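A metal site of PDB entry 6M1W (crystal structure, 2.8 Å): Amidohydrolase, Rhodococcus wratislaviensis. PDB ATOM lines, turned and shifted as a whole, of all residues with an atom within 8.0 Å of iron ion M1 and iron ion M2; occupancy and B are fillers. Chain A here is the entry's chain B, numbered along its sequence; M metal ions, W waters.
O of Tyr 338 lies within hydrogen-bond range of N of His 27, 2.8 Å away.
OE1 of Gln 106 sits close to OD1 of Asp 25, at 3.4 Å.
The side-chain carboxylate (OE2) of Glu 265 sits close to the side-chain amide oxygen (OE1) of Gln 309, 3.5 Å away.
The side-chain carboxylate of Asp 337 sits close to the side-chain amide oxygen of Gln 309 (3.2 Å).
ND1 of His 27 lies within hydrogen-bond range of O of Gln 106, at 2.6 Å.
Five residues have an atom within 4 Å of iron ion M1: Asp 25, His 27, His 211, Glu 265 and Asp 337.
Along chain A the residues within 4 Å of iron ion M1 span positions 25 to 337.
The nearest printed residue that does not touch iron ion M1 is His 340 (4.5 Å).
Within 4 Å of iron ion M2: Glu 265, Asp 337 and His 340.
The nearest printed residue that does not touch iron ion M2 is Asp 342 (4.3 Å).
Iron ion M1 is bound by a ring nitrogen (NE2) of His 211 (2.0 Å), the side-chain carboxylate of Asp 25 (2.2 Å), a ring nitrogen (NE2) of His 27 (2.2 Å), the side-chain carboxylate of Asp 337 (2.2 Å) and the side-chain carboxylate of Glu 265 (2.3 Å).
Iron ion M2 is bound by the side-chain carboxylate (OD2) of Asp 337, a ring nitrogen (ND1) of His 340, the side-chain carboxylate (OE2) of Glu 265 and the side-chain carboxylate (OE1) of Glu 265.
Slightly farther from iron ion M2 lies water W1 (2.7 Å).
Slightly farther from iron ion M2 lies water W2 (2.7 Å).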
ATOM      1  N   ALA A  24      -2.157 -17.956  35.237  1.00  0.00           N
ATOM      2  CA  ALA A  24      -3.063 -18.857  34.573  1.00  0.00           C
ATOM      3  C   ALA A  24      -2.343 -19.847  33.651  1.00  0.00           C
ATOM      4  O   ALA A  24      -3.030 -20.602  32.959  1.00  0.00           O
ATOM      5  CB  ALA A  24      -4.113 -18.053  33.794  1.00  0.00           C
ATOM      6  N   ASP A  25      -1.012 -19.893  33.633  1.00  0.00           N
ATOM      7  CA  ASP A  25      -0.310 -20.819  32.736  1.00  0.00           C
ATOM      8  C   ASP A  25       1.026 -21.229  33.351  1.00  0.00           C
ATOM      9  O   ASP A  25       2.042 -20.524  33.195  1.00  0.00           O
ATOM     10  CB  ASP A  25      -0.119 -20.186  31.365  1.00  0.00           C
ATOM     11  CG  ASP A  25       0.000 -21.212  30.267  1.00  0.00           C
ATOM     12  OD1 ASP A  25      -0.780 -22.183  30.263  1.00  0.00           O
ATOM     13  OD2 ASP A  25       0.835 -21.017  29.367  1.00  0.00           O
ATOM     14  N   ILE A  26       1.026 -22.382  34.021  1.00  0.00           N
ATOM     15  CA  ILE A  26       2.228 -23.049  34.523  1.00  0.00           C
ATOM     16  C   ILE A  26       2.370 -24.385  33.819  1.00  0.00           C
ATOM     17  O   ILE A  26       1.421 -25.179  33.825  1.00  0.00           O
ATOM     18  CB  ILE A  26       2.150 -23.303  36.040  1.00  0.00           C
ATOM     19  CG1 ILE A  26       1.974 -21.992  36.817  1.00  0.00           C
ATOM     20  CG2 ILE A  26       3.332 -24.165  36.482  1.00  0.00           C
ATOM     21  CD1 ILE A  26       3.231 -21.232  37.091  1.00  0.00           C
ATOM     22  N   HIS A  27       3.551 -24.650  33.259  1.00  0.00           N
ATOM     23  CA  HIS A  27       3.792 -25.927  32.591  1.00  0.00           C
ATOM     24  C   HIS A  27       4.674 -26.840  33.422  1.00  0.00           C
ATOM     25  O   HIS A  27       5.903 -26.723  33.372  1.00  0.00           O
ATOM     26  CB  HIS A  27       4.422 -25.711  31.212  1.00  0.00           C
ATOM     27  CG  HIS A  27       3.504 -25.074  30.227  1.00  0.00           C
ATOM     28  ND1 HIS A  27       2.278 -25.598  29.894  1.00  0.00           N
ATOM     29  CD2 HIS A  27       3.644 -23.954  29.490  1.00  0.00           C
ATOM     30  CE1 HIS A  27       1.688 -24.821  29.002  1.00  0.00           C
ATOM     31  NE2 HIS A  27       2.499 -23.811  28.743  1.00  0.00           N
ATOM     32  N   GLN A  66      10.571 -26.342  17.562  1.00  0.00           N
ATOM     33  CA  GLN A  66      11.356 -25.407  18.386  1.00  0.00           C
ATOM     34  C   GLN A  66      12.641 -24.999  17.675  1.00  0.00           C
ATOM     35  O   GLN A  66      13.292 -24.017  18.029  1.00  0.00           O
ATOM     36  CB  GLN A  66      11.706 -26.010  19.751  1.00  0.00           C
ATOM     37  CG  GLN A  66      10.760 -25.735  20.906  1.00  0.00           C
ATOM     38  CD  GLN A  66      10.961 -24.389  21.530  1.00  0.00           C
ATOM     39  OE1 GLN A  66      10.769 -23.348  20.885  1.00  0.00           O
ATOM     40  NE2 GLN A  66      11.366 -24.392  22.795  1.00  0.00           N
ATOM     41  N   GLN A 106      -1.107 -26.553  33.358  1.00  0.00           N
ATOM     42  CA  GLN A 106      -1.471 -26.839  31.979  1.00  0.00           C
ATOM     43  C   GLN A 106      -0.414 -27.787  31.458  1.00  0.00           C
ATOM     44  O   GLN A 106       0.590 -27.365  30.886  1.00  0.00           O
ATOM     45  CB  GLN A 106      -1.559 -25.539  31.180  1.00  0.00           C
ATOM     46  CG  GLN A 106      -2.516 -24.545  31.837  1.00  0.00           C
ATOM     47  CD  GLN A 106      -3.368 -23.756  30.850  1.00  0.00           C
ATOM     48  OE1 GLN A 106      -3.506 -24.121  29.678  1.00  0.00           O
ATOM     49  NE2 GLN A 106      -3.978 -22.690  31.338  1.00  0.00           N
ATOM     50  N   LEU A 108       0.654 -30.216  28.748  1.00  0.00           N
ATOM     51  CA  LEU A 108       0.372 -30.706  27.407  1.00  0.00           C
ATOM     52  C   LEU A 108       0.317 -32.233  27.400  1.00  0.00           C
ATOM     53  O   LEU A 108      -0.746 -32.830  27.185  1.00  0.00           O
ATOM     54  CB  LEU A 108       1.421 -30.186  26.419  1.00  0.00           C
ATOM     55  CG  LEU A 108       1.469 -28.662  26.269  1.00  0.00           C
ATOM     56  CD1 LEU A 108       0.069 -28.033  26.337  1.00  0.00           C
ATOM     57  CD2 LEU A 108       2.425 -28.025  27.284  1.00  0.00           C
ATOM     58  N   HIS A 211      -5.460 -23.597  25.127  1.00  0.00           N
ATOM     59  CA  HIS A 211      -4.061 -23.244  25.129  1.00  0.00           C
ATOM     60  C   HIS A 211      -3.465 -23.436  23.732  1.00  0.00           C
ATOM     61  O   HIS A 211      -3.766 -24.436  23.054  1.00  0.00           O
ATOM     62  CB  HIS A 211      -3.312 -24.109  26.143  1.00  0.00           C
ATOM     63  CG  HIS A 211      -1.890 -23.705  26.353  1.00  0.00           C
ATOM     64  ND1 HIS A 211      -0.888 -23.979  25.446  1.00  0.00           N
ATOM     65  CD2 HIS A 211      -1.287 -23.057  27.388  1.00  0.00           C
ATOM     66  CE1 HIS A 211       0.253 -23.507  25.893  1.00  0.00           C
ATOM     67  NE2 HIS A 211       0.036 -22.943  27.076  1.00  0.00           N
ATOM     68  N   LEU A 212      -2.601 -22.488  23.351  1.00  0.00           N
ATOM     69  CA  LEU A 212      -1.890 -22.487  22.079  1.00  0.00           C
ATOM     70  C   LEU A 212      -1.434 -23.885  21.708  1.00  0.00           C
ATOM     71  O   LEU A 212      -0.981 -24.653  22.570  1.00  0.00           O
ATOM     72  CB  LEU A 212      -0.695 -21.535  22.181  1.00  0.00           C
ATOM     73  CG  LEU A 212       0.474 -21.536  21.191  1.00  0.00           C
ATOM     74  CD1 LEU A 212       1.047 -20.159  21.104  1.00  0.00           C
ATOM     75  CD2 LEU A 212       1.587 -22.492  21.582  1.00  0.00           C
ATOM     76  N   HIS A 233       5.494 -18.965  14.853  1.00  0.00           N
ATOM     77  CA  HIS A 233       5.169 -18.449  16.174  1.00  0.00           C
ATOM     78  C   HIS A 233       4.104 -17.352  16.114  1.00  0.00           C
ATOM     79  O   HIS A 233       3.151 -17.364  16.901  1.00  0.00           O
ATOM     80  CB  HIS A 233       6.436 -17.938  16.882  1.00  0.00           C
ATOM     81  CG  HIS A 233       6.461 -18.202  18.364  1.00  0.00           C
ATOM     82  ND1 HIS A 233       7.399 -19.018  18.951  1.00  0.00           N
ATOM     83  CD2 HIS A 233       5.655 -17.755  19.349  1.00  0.00           C
ATOM     84  CE1 HIS A 233       7.166 -19.067  20.252  1.00  0.00           C
ATOM     85  NE2 HIS A 233       6.122 -18.310  20.526  1.00  0.00           N
ATOM     86  N   VAL A 264      -5.293 -18.732  25.911  1.00  0.00           N
ATOM     87  CA  VAL A 264      -4.039 -18.763  26.638  1.00  0.00           C
ATOM     88  C   VAL A 264      -2.873 -18.847  25.652  1.00  0.00           C
ATOM     89  O   VAL A 264      -2.927 -19.594  24.681  1.00  0.00           O
ATOM     90  CB  VAL A 264      -3.978 -19.953  27.619  1.00  0.00           C
ATOM     91  CG1 VAL A 264      -2.750 -19.844  28.471  1.00  0.00           C
ATOM     92  CG2 VAL A 264      -5.228 -20.010  28.474  1.00  0.00           C
ATOM     93  N   GLU A 265      -1.813 -18.095  25.946  1.00  0.00           N
ATOM     94  CA  GLU A 265      -0.619 -17.940  25.108  1.00  0.00           C
ATOM     95  C   GLU A 265      -1.009 -17.455  23.712  1.00  0.00           C
ATOM     96  O   GLU A 265      -0.331 -17.741  22.712  1.00  0.00           O
ATOM     97  CB  GLU A 265       0.243 -19.213  25.095  1.00  0.00           C
ATOM     98  CG  GLU A 265       1.619 -19.020  24.441  1.00  0.00           C
ATOM     99  CD  GLU A 265       2.738 -19.764  25.093  1.00  0.00           C
ATOM    100  OE1 GLU A 265       2.449 -20.568  25.996  1.00  0.00           O
ATOM    101  OE2 GLU A 265       3.903 -19.542  24.670  1.00  0.00           O
ATOM    102  N   GLY A 266      -2.126 -16.755  23.606  1.00  0.00           N
ATOM    103  CA  GLY A 266      -2.585 -16.252  22.325  1.00  0.00           C
ATOM    104  C   GLY A 266      -2.444 -14.773  22.043  1.00  0.00           C
ATOM    105  O   GLY A 266      -2.845 -14.349  20.949  1.00  0.00           O
ATOM    106  N   SER A 307      -5.292 -14.789  28.573  1.00  0.00           N
ATOM    107  CA  SER A 307      -3.993 -14.742  29.231  1.00  0.00           C
ATOM    108  C   SER A 307      -3.110 -13.687  28.605  1.00  0.00           C
ATOM    109  O   SER A 307      -3.271 -13.337  27.438  1.00  0.00           O
ATOM    110  CB  SER A 307      -3.315 -16.116  29.152  1.00  0.00           C
ATOM    111  OG  SER A 307      -1.900 -16.097  29.054  1.00  0.00           O
ATOM    112  N   GLN A 309       0.399 -13.728  28.479  1.00  0.00           N
ATOM    113  CA  GLN A 309       1.698 -14.130  27.978  1.00  0.00           C
ATOM    114  C   GLN A 309       1.563 -14.620  26.533  1.00  0.00           C
ATOM    115  O   GLN A 309       0.589 -15.299  26.209  1.00  0.00           O
ATOM    116  CB  GLN A 309       2.270 -15.246  28.854  1.00  0.00           C
ATOM    117  CG  GLN A 309       3.750 -15.468  28.672  1.00  0.00           C
ATOM    118  CD  GLN A 309       4.045 -16.461  27.559  1.00  0.00           C
ATOM    119  OE1 GLN A 309       3.304 -17.435  27.370  1.00  0.00           O
ATOM    120  NE2 GLN A 309       5.112 -16.211  26.812  1.00  0.00           N
ATOM    121  N   PRO A 310       2.496 -14.257  25.641  1.00  0.00           N
ATOM    122  CA  PRO A 310       3.566 -13.276  25.867  1.00  0.00           C
ATOM    123  C   PRO A 310       3.048 -11.841  25.733  1.00  0.00           C
ATOM    124  O   PRO A 310       2.160 -11.564  24.917  1.00  0.00           O
ATOM    125  CB  PRO A 310       4.573 -13.600  24.766  1.00  0.00           C
ATOM    126  CG  PRO A 310       3.722 -14.143  23.631  1.00  0.00           C
ATOM    127  CD  PRO A 310       2.590 -14.894  24.302  1.00  0.00           C
ATOM    128  N   ALA A 335      -0.228 -14.372  33.187  1.00  0.00           N
ATOM    129  CA  ALA A 335       0.438 -15.667  33.027  1.00  0.00           C
ATOM    130  C   ALA A 335       1.931 -15.435  32.848  1.00  0.00           C
ATOM    131  O   ALA A 335       2.346 -14.398  32.308  1.00  0.00           O
ATOM    132  CB  ALA A 335      -0.115 -16.449  31.835  1.00  0.00           C
ATOM    133  N   THR A 336       2.735 -16.398  33.326  1.00  0.00           N
ATOM    134  CA  THR A 336       4.175 -16.432  33.082  1.00  0.00           C
ATOM    135  C   THR A 336       4.572 -17.338  31.932  1.00  0.00           C
ATOM    136  O   THR A 336       5.503 -16.994  31.193  1.00  0.00           O
ATOM    137  CB  THR A 336       4.938 -16.931  34.314  1.00  0.00           C
ATOM    138  OG1 THR A 336       4.409 -16.340  35.507  1.00  0.00           O
ATOM    139  CG2 THR A 336       6.439 -16.621  34.206  1.00  0.00           C
ATOM    140  N   ASP A 337       3.919 -18.501  31.808  1.00  0.00           N
ATOM    141  CA  ASP A 337       4.456 -19.603  31.024  1.00  0.00           C
ATOM    142  C   ASP A 337       5.829 -19.981  31.572  1.00  0.00           C
ATOM    143  O   ASP A 337       6.869 -19.841  30.913  1.00  0.00           O
ATOM    144  CB  ASP A 337       4.509 -19.234  29.533  1.00  0.00           C
ATOM    145  CG  ASP A 337       4.089 -20.357  28.608  1.00  0.00           C
ATOM    146  OD1 ASP A 337       3.337 -21.251  29.022  1.00  0.00           O
ATOM    147  OD2 ASP A 337       4.533 -20.348  27.472  1.00  0.00           O
ATOM    148  N   TYR A 338       5.825 -20.375  32.804  1.00  0.00           N
ATOM    149  CA  TYR A 338       6.974 -21.112  33.313  1.00  0.00           C
ATOM    150  C   TYR A 338       6.899 -22.551  32.805  1.00  0.00           C
ATOM    151  O   TYR A 338       5.814 -23.153  32.787  1.00  0.00           O
ATOM    152  CB  TYR A 338       6.983 -21.095  34.840  1.00  0.00           C
ATOM    153  CG  TYR A 338       8.322 -21.454  35.436  1.00  0.00           C
ATOM    154  CD1 TYR A 338       9.408 -20.593  35.345  1.00  0.00           C
ATOM    155  CD2 TYR A 338       8.500 -22.665  36.098  1.00  0.00           C
ATOM    156  CE1 TYR A 338      10.647 -20.933  35.893  1.00  0.00           C
ATOM    157  CE2 TYR A 338       9.722 -23.018  36.653  1.00  0.00           C
ATOM    158  CZ  TYR A 338      10.797 -22.132  36.546  1.00  0.00           C
ATOM    159  OH  TYR A 338      12.019 -22.474  37.091  1.00  0.00           O
ATOM    160  N   PRO A 339       8.030 -23.139  32.396  1.00  0.00           N
ATOM    161  CA  PRO A 339       9.366 -22.537  32.368  1.00  0.00           C
ATOM    162  C   PRO A 339       9.824 -22.066  30.988  1.00  0.00           C
ATOM    163  O   PRO A 339      11.029 -21.987  30.735  1.00  0.00           O
ATOM    164  CB  PRO A 339      10.245 -23.677  32.860  1.00  0.00           C
ATOM    165  CG  PRO A 339       9.579 -24.913  32.261  1.00  0.00           C
ATOM    166  CD  PRO A 339       8.099 -24.584  32.075  1.00  0.00           C
ATOM    167  N   HIS A 340       8.869 -21.765  30.100  1.00  0.00           N
ATOM    168  CA  HIS A 340       9.179 -21.512  28.698  1.00  0.00           C
ATOM    169  C   HIS A 340      10.105 -20.309  28.534  1.00  0.00           C
ATOM    170  O   HIS A 340      10.175 -19.408  29.381  1.00  0.00           O
ATOM    171  CB  HIS A 340       7.901 -21.301  27.891  1.00  0.00           C
ATOM    172  CG  HIS A 340       7.170 -22.570  27.540  1.00  0.00           C
ATOM    173  ND1 HIS A 340       6.146 -22.615  26.626  1.00  0.00           N
ATOM    174  CD2 HIS A 340       7.320 -23.835  28.001  1.00  0.00           C
ATOM    175  CE1 HIS A 340       5.698 -23.855  26.526  1.00  0.00           C
ATOM    176  NE2 HIS A 340       6.398 -24.609  27.347  1.00  0.00           N
ATOM    177  N   PHE A 341      10.824 -20.285  27.399  1.00  0.00           N
ATOM    178  CA  PHE A 341      11.862 -19.290  27.169  1.00  0.00           C
ATOM    179  C   PHE A 341      11.302 -17.870  27.149  1.00  0.00           C
ATOM    180  O   PHE A 341      11.985 -16.926  27.548  1.00  0.00           O
ATOM    181  CB  PHE A 341      12.625 -19.601  25.873  1.00  0.00           C
ATOM    182  CG  PHE A 341      12.028 -18.981  24.624  1.00  0.00           C
ATOM    183  CD1 PHE A 341      12.409 -17.696  24.216  1.00  0.00           C
ATOM    184  CD2 PHE A 341      11.126 -19.680  23.844  1.00  0.00           C
ATOM    185  CE1 PHE A 341      11.878 -17.120  23.058  1.00  0.00           C
ATOM    186  CE2 PHE A 341      10.584 -19.113  22.686  1.00  0.00           C
ATOM    187  CZ  PHE A 341      10.962 -17.824  22.292  1.00  0.00           C
ATOM    188  N   ASP A 342      10.052 -17.701  26.708  1.00  0.00           N
ATOM    189  CA  ASP A 342       9.434 -16.389  26.584  1.00  0.00           C
ATOM    190  C   ASP A 342       8.574 -16.062  27.789  1.00  0.00           C
ATOM    191  O   ASP A 342       7.506 -15.452  27.663  1.00  0.00           O
ATOM    192  CB  ASP A 342       8.624 -16.259  25.293  1.00  0.00           C
ATOM    193  CG  ASP A 342       7.746 -17.487  24.975  1.00  0.00           C
ATOM    194  OD1 ASP A 342       7.965 -18.593  25.545  1.00  0.00           O
ATOM    195  OD2 ASP A 342       6.839 -17.341  24.113  1.00  0.00           O
ATOM    196  N   PHE A 343       9.015 -16.467  28.975  1.00  0.00           N
ATOM    197  CA  PHE A 343       8.343 -16.133  30.210  1.00  0.00           C
ATOM    198  C   PHE A 343       8.460 -14.633  30.518  1.00  0.00           C
ATOM    199  O   PHE A 343       9.397 -13.957  30.093  1.00  0.00           O
ATOM    200  CB  PHE A 343       8.930 -16.937  31.368  1.00  0.00           C
ATOM    201  CG  PHE A 343      10.146 -16.324  31.967  1.00  0.00           C
ATOM    202  CD1 PHE A 343      11.327 -16.240  31.217  1.00  0.00           C
ATOM    203  CD2 PHE A 343      10.114 -15.780  33.252  1.00  0.00           C
ATOM    204  CE1 PHE A 343      12.456 -15.655  31.760  1.00  0.00           C
ATOM    205  CE2 PHE A 343      11.243 -15.195  33.795  1.00  0.00           C
ATOM    206  CZ  PHE A 343      12.419 -15.128  33.049  1.00  0.00           C
HETATM  207 FE    FE M   1       1.777 -22.030  27.650  1.00  0.00          FE
HETATM  208 FE    FE M   2       4.735 -21.354  25.727  1.00  0.00          FE
HETATM  209  O   HOH W   1       4.432 -23.294  23.809  1.00  0.00           O
HETATM  210  O   HOH W   2       6.564 -20.748  23.765  1.00  0.00           O
